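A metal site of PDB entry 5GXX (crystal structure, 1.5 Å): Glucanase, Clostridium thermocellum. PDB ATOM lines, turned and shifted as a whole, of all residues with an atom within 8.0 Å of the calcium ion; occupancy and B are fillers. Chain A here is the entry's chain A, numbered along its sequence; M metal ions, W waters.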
ATOM      1  N   LEU A  59     -16.049  15.832  13.520  1.00  0.00           N
ATOM      2  CA  LEU A  59     -17.494  16.005  13.695  1.00  0.00           C
ATOM      3  C   LEU A  59     -18.247  15.591  12.426  1.00  0.00           C
ATOM      4  O   LEU A  59     -19.065  14.677  12.486  1.00  0.00           O
ATOM      5  CB  LEU A  59     -17.891  17.404  14.209  1.00  0.00           C
ATOM      6  CG  LEU A  59     -19.381  17.688  14.442  1.00  0.00           C
ATOM      7  CD1 LEU A  59     -20.025  16.679  15.396  1.00  0.00           C
ATOM      8  CD2 LEU A  59     -19.550  19.105  14.970  1.00  0.00           C
ATOM      9  N   SER A 142     -18.133  17.802  23.789  1.00  0.00           N
ATOM     10  CA  SER A 142     -19.295  16.924  23.887  1.00  0.00           C
ATOM     11  C   SER A 142     -19.927  16.634  22.513  1.00  0.00           C
ATOM     12  O   SER A 142     -20.341  15.500  22.271  1.00  0.00           O
ATOM     13  CB  SER A 142     -20.307  17.438  24.916  1.00  0.00           C
ATOM     14  OG  SER A 142     -19.813  17.373  26.269  1.00  0.00           O
ATOM     15  N   ALA A 143     -19.999  17.637  21.638  1.00  0.00           N
ATOM     16  CA  ALA A 143     -20.562  17.441  20.296  1.00  0.00           C
ATOM     17  C   ALA A 143     -19.724  16.464  19.471  1.00  0.00           C
ATOM     18  O   ALA A 143     -20.212  15.433  19.012  1.00  0.00           O
ATOM     19  CB  ALA A 143     -20.703  18.769  19.563  1.00  0.00           C
ATOM     20  N   VAL A 144     -18.430  16.747  19.348  1.00  0.00           N
ATOM     21  CA  VAL A 144     -17.590  15.875  18.536  1.00  0.00           C
ATOM     22  C   VAL A 144     -17.476  14.479  19.150  1.00  0.00           C
ATOM     23  O   VAL A 144     -17.609  13.477  18.427  1.00  0.00           O
ATOM     24  CB  VAL A 144     -16.223  16.496  18.176  1.00  0.00           C
ATOM     25  CG1 VAL A 144     -15.321  16.646  19.409  1.00  0.00           C
ATOM     26  CG2 VAL A 144     -15.528  15.707  17.069  1.00  0.00           C
ATOM     27  N   GLN A 147     -20.846  12.588  18.792  1.00  0.00           N
ATOM     28  CA  GLN A 147     -21.038  12.115  17.410  1.00  0.00           C
ATOM     29  C   GLN A 147     -20.163  10.897  17.111  1.00  0.00           C
ATOM     30  O   GLN A 147     -20.620   9.946  16.468  1.00  0.00           O
ATOM     31  CB  GLN A 147     -20.813  13.245  16.390  1.00  0.00           C
ATOM     32  CG  GLN A 147     -21.227  12.910  14.943  1.00  0.00           C
ATOM     33  CD  GLN A 147     -22.696  12.563  14.788  1.00  0.00           C
ATOM     34  OE1 GLN A 147     -23.022  11.457  14.362  1.00  0.00           O
ATOM     35  NE2 GLN A 147     -23.584  13.480  15.137  1.00  0.00           N
ATOM     36  N   ASP A 181     -18.621  22.119  25.019  1.00  0.00           N
ATOM     37  CA  ASP A 181     -17.893  22.214  23.764  1.00  0.00           C
ATOM     38  C   ASP A 181     -16.659  23.105  23.875  1.00  0.00           C
ATOM     39  O   ASP A 181     -16.055  23.440  22.862  1.00  0.00           O
ATOM     40  CB  ASP A 181     -18.817  22.751  22.673  1.00  0.00           C
ATOM     41  CG  ASP A 181     -19.728  21.682  22.107  1.00  0.00           C
ATOM     42  OD1 ASP A 181     -19.333  20.499  22.052  1.00  0.00           O
ATOM     43  OD2 ASP A 181     -20.861  22.048  21.719  1.00  0.00           O
ATOM     44  N   SER A 192     -17.886  24.735  13.320  1.00  0.00           N
ATOM     45  CA  SER A 192     -18.241  25.234  14.647  1.00  0.00           C
ATOM     46  C   SER A 192     -19.477  24.510  15.191  1.00  0.00           C
ATOM     47  O   SER A 192     -20.360  24.155  14.397  1.00  0.00           O
ATOM     48  CB  SER A 192     -18.501  26.738  14.584  1.00  0.00           C
ATOM     49  OG  SER A 192     -17.281  27.470  14.482  1.00  0.00           O
ATOM     50  N   SER A 193     -19.517  24.267  16.504  1.00  0.00           N
ATOM     51  CA  SER A 193     -20.716  23.713  17.121  1.00  0.00           C
ATOM     52  C   SER A 193     -21.746  24.841  17.248  1.00  0.00           C
ATOM     53  O   SER A 193     -21.597  25.745  18.070  1.00  0.00           O
ATOM     54  CB  SER A 193     -20.395  23.083  18.493  1.00  0.00           C
ATOM     55  OG  SER A 193     -21.558  22.537  19.103  1.00  0.00           O
ATOM     56  N   HIS A 194     -22.766  24.816  16.396  1.00  0.00           N
ATOM     57  CA  HIS A 194     -23.775  25.880  16.368  1.00  0.00           C
ATOM     58  C   HIS A 194     -24.924  25.614  17.324  1.00  0.00           C
ATOM     59  O   HIS A 194     -25.384  26.501  18.047  1.00  0.00           O
ATOM     60  CB  HIS A 194     -24.331  26.049  14.951  1.00  0.00           C
ATOM     61  CG  HIS A 194     -23.279  26.357  13.940  1.00  0.00           C
ATOM     62  ND1 HIS A 194     -22.610  27.565  13.914  1.00  0.00           N
ATOM     63  CD2 HIS A 194     -22.728  25.600  12.956  1.00  0.00           C
ATOM     64  CE1 HIS A 194     -21.715  27.547  12.938  1.00  0.00           C
ATOM     65  NE2 HIS A 194     -21.759  26.360  12.349  1.00  0.00           N
ATOM     66  N   SER A 195     -25.424  24.378  17.301  1.00  0.00           N
ATOM     67  CA  SER A 195     -26.625  24.018  18.025  1.00  0.00           C
ATOM     68  C   SER A 195     -26.310  23.657  19.479  1.00  0.00           C
ATOM     69  O   SER A 195     -27.220  23.464  20.276  1.00  0.00           O
ATOM     70  CB  SER A 195     -27.327  22.832  17.351  1.00  0.00           C
ATOM     71  OG  SER A 195     -26.407  21.760  17.157  1.00  0.00           O
ATOM     72  N   GLY A 196     -25.029  23.525  19.827  1.00  0.00           N
ATOM     73  CA  GLY A 196     -24.657  22.981  21.118  1.00  0.00           C
ATOM     74  C   GLY A 196     -24.507  21.479  21.057  1.00  0.00           C
ATOM     75  O   GLY A 196     -24.485  20.879  19.971  1.00  0.00           O
ATOM     76  N   PHE A 197     -24.441  20.868  22.237  1.00  0.00           N
ATOM     77  CA  PHE A 197     -24.081  19.458  22.345  1.00  0.00           C
ATOM     78  C   PHE A 197     -25.213  18.549  22.843  1.00  0.00           C
ATOM     79  O   PHE A 197     -25.059  17.333  22.834  1.00  0.00           O
ATOM     80  CB  PHE A 197     -22.822  19.317  23.216  1.00  0.00           C
ATOM     81  CG  PHE A 197     -23.053  19.724  24.655  1.00  0.00           C
ATOM     82  CD1 PHE A 197     -23.849  18.932  25.465  1.00  0.00           C
ATOM     83  CD2 PHE A 197     -22.557  20.923  25.154  1.00  0.00           C
ATOM     84  CE1 PHE A 197     -24.118  19.274  26.783  1.00  0.00           C
ATOM     85  CE2 PHE A 197     -22.839  21.291  26.478  1.00  0.00           C
ATOM     86  CZ  PHE A 197     -23.631  20.476  27.281  1.00  0.00           C
ATOM     87  N   TRP A 198     -26.344  19.117  23.249  1.00  0.00           N
ATOM     88  CA  TRP A 198     -27.456  18.285  23.713  1.00  0.00           C
ATOM     89  C   TRP A 198     -27.995  17.349  22.626  1.00  0.00           C
ATOM     90  O   TRP A 198     -28.378  16.209  22.913  1.00  0.00           O
ATOM     91  CB  TRP A 198     -28.572  19.120  24.355  1.00  0.00           C
ATOM     92  CG  TRP A 198     -28.131  19.883  25.574  1.00  0.00           C
ATOM     93  CD1 TRP A 198     -28.010  21.230  25.686  1.00  0.00           C
ATOM     94  CD2 TRP A 198     -27.747  19.334  26.846  1.00  0.00           C
ATOM     95  NE1 TRP A 198     -27.579  21.575  26.953  1.00  0.00           N
ATOM     96  CE2 TRP A 198     -27.407  20.427  27.678  1.00  0.00           C
ATOM     97  CE3 TRP A 198     -27.653  18.028  27.361  1.00  0.00           C
ATOM     98  CZ2 TRP A 198     -26.991  20.250  29.009  1.00  0.00           C
ATOM     99  CZ3 TRP A 198     -27.242  17.862  28.681  1.00  0.00           C
ATOM    100  CH2 TRP A 198     -26.919  18.960  29.490  1.00  0.00           C
ATOM    101  N   ASP A 199     -28.068  17.823  21.385  1.00  0.00           N
ATOM    102  CA  ASP A 199     -28.518  16.962  20.303  1.00  0.00           C
ATOM    103  C   ASP A 199     -27.600  15.762  20.047  1.00  0.00           C
ATOM    104  O   ASP A 199     -28.090  14.674  19.773  1.00  0.00           O
ATOM    105  CB  ASP A 199     -28.701  17.779  19.004  1.00  0.00           C
ATOM    106  CG  ASP A 199     -27.468  18.605  18.655  1.00  0.00           C
ATOM    107  OD1 ASP A 199     -27.272  19.667  19.291  1.00  0.00           O
ATOM    108  OD2 ASP A 199     -26.710  18.212  17.750  1.00  0.00           O
ATOM    109  N   GLU A 200     -26.283  15.948  20.135  1.00  0.00           N
ATOM    110  CA  GLU A 200     -25.372  14.807  19.996  1.00  0.00           C
ATOM    111  C   GLU A 200     -25.561  13.795  21.123  1.00  0.00           C
ATOM    112  O   GLU A 200     -25.481  12.588  20.903  1.00  0.00           O
ATOM    113  CB  GLU A 200     -23.893  15.231  19.965  1.00  0.00           C
ATOM    114  CG  GLU A 200     -23.424  15.942  18.698  1.00  0.00           C
ATOM    115  CD  GLU A 200     -23.863  17.379  18.609  1.00  0.00           C
ATOM    116  OE1 GLU A 200     -24.397  17.909  19.611  1.00  0.00           O
ATOM    117  OE2 GLU A 200     -23.652  18.005  17.541  1.00  0.00           O
ATOM    118  N   LEU A 201     -25.789  14.279  22.335  1.00  0.00           N
ATOM    119  CA  LEU A 201     -26.016  13.332  23.434  1.00  0.00           C
ATOM    120  C   LEU A 201     -27.298  12.538  23.220  1.00  0.00           C
ATOM    121  O   LEU A 201     -27.326  11.340  23.491  1.00  0.00           O
ATOM    122  CB  LEU A 201     -26.010  14.006  24.810  1.00  0.00           C
ATOM    123  CG  LEU A 201     -24.704  14.670  25.227  1.00  0.00           C
ATOM    124  CD1 LEU A 201     -24.943  15.343  26.596  1.00  0.00           C
ATOM    125  CD2 LEU A 201     -23.570  13.650  25.307  1.00  0.00           C
ATOM    126  N   LEU A 228     -32.991  20.674  24.315  1.00  0.00           N
ATOM    127  CA  LEU A 228     -32.816  20.996  22.910  1.00  0.00           C
ATOM    128  C   LEU A 228     -33.280  22.416  22.658  1.00  0.00           C
ATOM    129  O   LEU A 228     -34.142  22.933  23.381  1.00  0.00           O
ATOM    130  CB  LEU A 228     -33.613  20.037  22.017  1.00  0.00           C
ATOM    131  CG  LEU A 228     -33.204  18.566  22.085  1.00  0.00           C
ATOM    132  CD1 LEU A 228     -34.245  17.717  21.368  1.00  0.00           C
ATOM    133  CD2 LEU A 228     -31.818  18.318  21.535  1.00  0.00           C
ATOM    134  N   ASN A 229     -32.712  23.047  21.631  1.00  0.00           N
ATOM    135  CA  ASN A 229     -33.119  24.391  21.239  1.00  0.00           C
ATOM    136  C   ASN A 229     -34.586  24.448  20.824  1.00  0.00           C
ATOM    137  O   ASN A 229     -35.150  23.463  20.343  1.00  0.00           O
ATOM    138  CB  ASN A 229     -32.196  24.941  20.147  1.00  0.00           C
ATOM    139  CG  ASN A 229     -30.722  24.861  20.533  1.00  0.00           C
ATOM    140  OD1 ASN A 229     -29.892  24.384  19.754  1.00  0.00           O
ATOM    141  ND2 ASN A 229     -30.403  25.295  21.751  1.00  0.00           N
ATOM    142  N   CYS A 244     -28.217  17.200  10.080  1.00  0.00           N
ATOM    143  CA  CYS A 244     -26.904  17.431   9.468  1.00  0.00           C
ATOM    144  C   CYS A 244     -25.776  17.211  10.471  1.00  0.00           C
ATOM    145  O   CYS A 244     -26.027  16.920  11.653  1.00  0.00           O
ATOM    146  CB  CYS A 244     -26.847  18.865   8.942  1.00  0.00           C
ATOM    147  SG  CYS A 244     -26.929  20.158  10.236  1.00  0.00           S
ATOM    148  N   TRP A 245     -24.550  17.402  10.003  1.00  0.00           N
ATOM    149  CA  TRP A 245     -23.351  17.196  10.841  1.00  0.00           C
ATOM    150  C   TRP A 245     -23.395  17.927  12.178  1.00  0.00           C
ATOM    151  O   TRP A 245     -22.770  17.456  13.130  1.00  0.00           O
ATOM    152  CB  TRP A 245     -22.068  17.570  10.095  1.00  0.00           C
ATOM    153  CG  TRP A 245     -22.061  19.025   9.683  1.00  0.00           C
ATOM    154  CD1 TRP A 245     -22.527  19.562   8.513  1.00  0.00           C
ATOM    155  CD2 TRP A 245     -21.624  20.136  10.474  1.00  0.00           C
ATOM    156  NE1 TRP A 245     -22.407  20.928   8.523  1.00  0.00           N
ATOM    157  CE2 TRP A 245     -21.836  21.307   9.713  1.00  0.00           C
ATOM    158  CE3 TRP A 245     -21.058  20.255  11.751  1.00  0.00           C
ATOM    159  CZ2 TRP A 245     -21.522  22.588  10.185  1.00  0.00           C
ATOM    160  CZ3 TRP A 245     -20.736  21.523  12.215  1.00  0.00           C
ATOM    161  CH2 TRP A 245     -20.975  22.671  11.443  1.00  0.00           C
ATOM    162  N   ASP A 246     -24.050  19.073  12.246  1.00  0.00           N
ATOM    163  CA  ASP A 246     -24.091  19.885  13.456  1.00  0.00           C
ATOM    164  C   ASP A 246     -25.199  19.501  14.445  1.00  0.00           C
ATOM    165  O   ASP A 246     -25.137  19.801  15.652  1.00  0.00           O
ATOM    166  CB  ASP A 246     -24.258  21.348  13.084  1.00  0.00           C
ATOM    167  CG  ASP A 246     -24.213  22.257  14.287  1.00  0.00           C
ATOM    168  OD1 ASP A 246     -23.124  22.408  14.866  1.00  0.00           O
ATOM    169  OD2 ASP A 246     -25.282  22.782  14.683  1.00  0.00           O
ATOM    170  N   ASP A 247     -26.234  18.866  13.906  1.00  0.00           N
ATOM    171  CA  ASP A 247     -27.474  18.667  14.614  1.00  0.00           C
ATOM    172  C   ASP A 247     -28.308  17.498  14.085  1.00  0.00           C
ATOM    173  O   ASP A 247     -28.975  17.590  13.053  1.00  0.00           O
ATOM    174  CB  ASP A 247     -28.287  19.970  14.593  1.00  0.00           C
ATOM    175  CG  ASP A 247     -29.468  19.948  15.538  1.00  0.00           C
ATOM    176  OD1 ASP A 247     -29.754  18.879  16.144  1.00  0.00           O
ATOM    177  OD2 ASP A 247     -30.126  21.001  15.632  1.00  0.00           O
ATOM    178  N   CYS A 248     -28.250  16.401  14.833  1.00  0.00           N
ATOM    179  CA  CYS A 248     -28.934  15.167  14.527  1.00  0.00           C
ATOM    180  C   CYS A 248     -30.198  14.948  15.355  1.00  0.00           C
ATOM    181  O   CYS A 248     -30.733  13.841  15.360  1.00  0.00           O
ATOM    182  CB  CYS A 248     -27.963  13.983  14.700  1.00  0.00           C
ATOM    183  SG  CYS A 248     -26.709  13.833  13.422  1.00  0.00           S
ATOM    184  N   HIS A 249     -30.709  15.957  16.054  1.00  0.00           N
ATOM    185  CA  HIS A 249     -31.907  15.736  16.860  1.00  0.00           C
ATOM    186  C   HIS A 249     -33.114  15.353  16.031  1.00  0.00           C
ATOM    187  O   HIS A 249     -33.966  14.601  16.500  1.00  0.00           O
ATOM    188  CB  HIS A 249     -32.264  16.830  17.884  1.00  0.00           C
ATOM    189  CG  HIS A 249     -32.972  18.028  17.316  1.00  0.00           C
ATOM    190  ND1 HIS A 249     -32.292  19.113  16.825  1.00  0.00           N
ATOM    191  CD2 HIS A 249     -34.293  18.352  17.263  1.00  0.00           C
ATOM    192  CE1 HIS A 249     -33.160  20.044  16.449  1.00  0.00           C
ATOM    193  NE2 HIS A 249     -34.379  19.591  16.683  1.00  0.00           N
HETATM  194 CA    CA M   1     -25.040  19.816  17.993  1.00  0.00          CA
HETATM  195  O   HOH W   1     -23.266  21.128  17.461  1.00  0.00           O
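The side-chain sulfur of Cys 244 sits close to the backbone NH of Asp 246 (3.7 Å).
The backbone carbonyl oxygen (O) of Ser 195 lies close to the side-chain amide oxygen (OD1) of Asn 229.
O of Gly 196 sits close to OG of Ser 193, 3.5 Å away.
The backbone NH (N) of His 194 lies within hydrogen-bond range of the side-chain carboxylate (OD1) of Asp 246, 2.9 Å away.
Of the 24 residues printed, 5 come within 4 Å of the calcium ion.
The calcium ion is bound by water W1 (2.3 Å).
The calcium ion is bound by O of Gly 196, 2.3 Å away.
The calcium ion is bound by OE2 of Glu 200 (2.3 Å).
The side-chain carboxylate (OD2) of Asp 199 binds the calcium ion, at 2.3 Å.
The backbone carbonyl oxygen (O) of Asp 246 is bound to the calcium ion.
OG of Ser 195 is bound to the calcium ion, 2.5 Å away.
OE1 of Glu 200 is bound to the calcium ion (2.6 Å).
The calcium ion is bound by OD1 of Asp 199 (2.6 Å).
The calcium ion has eight donor atoms within binding distance.
Water W1 bridges the side-chain hydroxyl of Ser 193 and the side-chain carboxylate of Asp 246.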
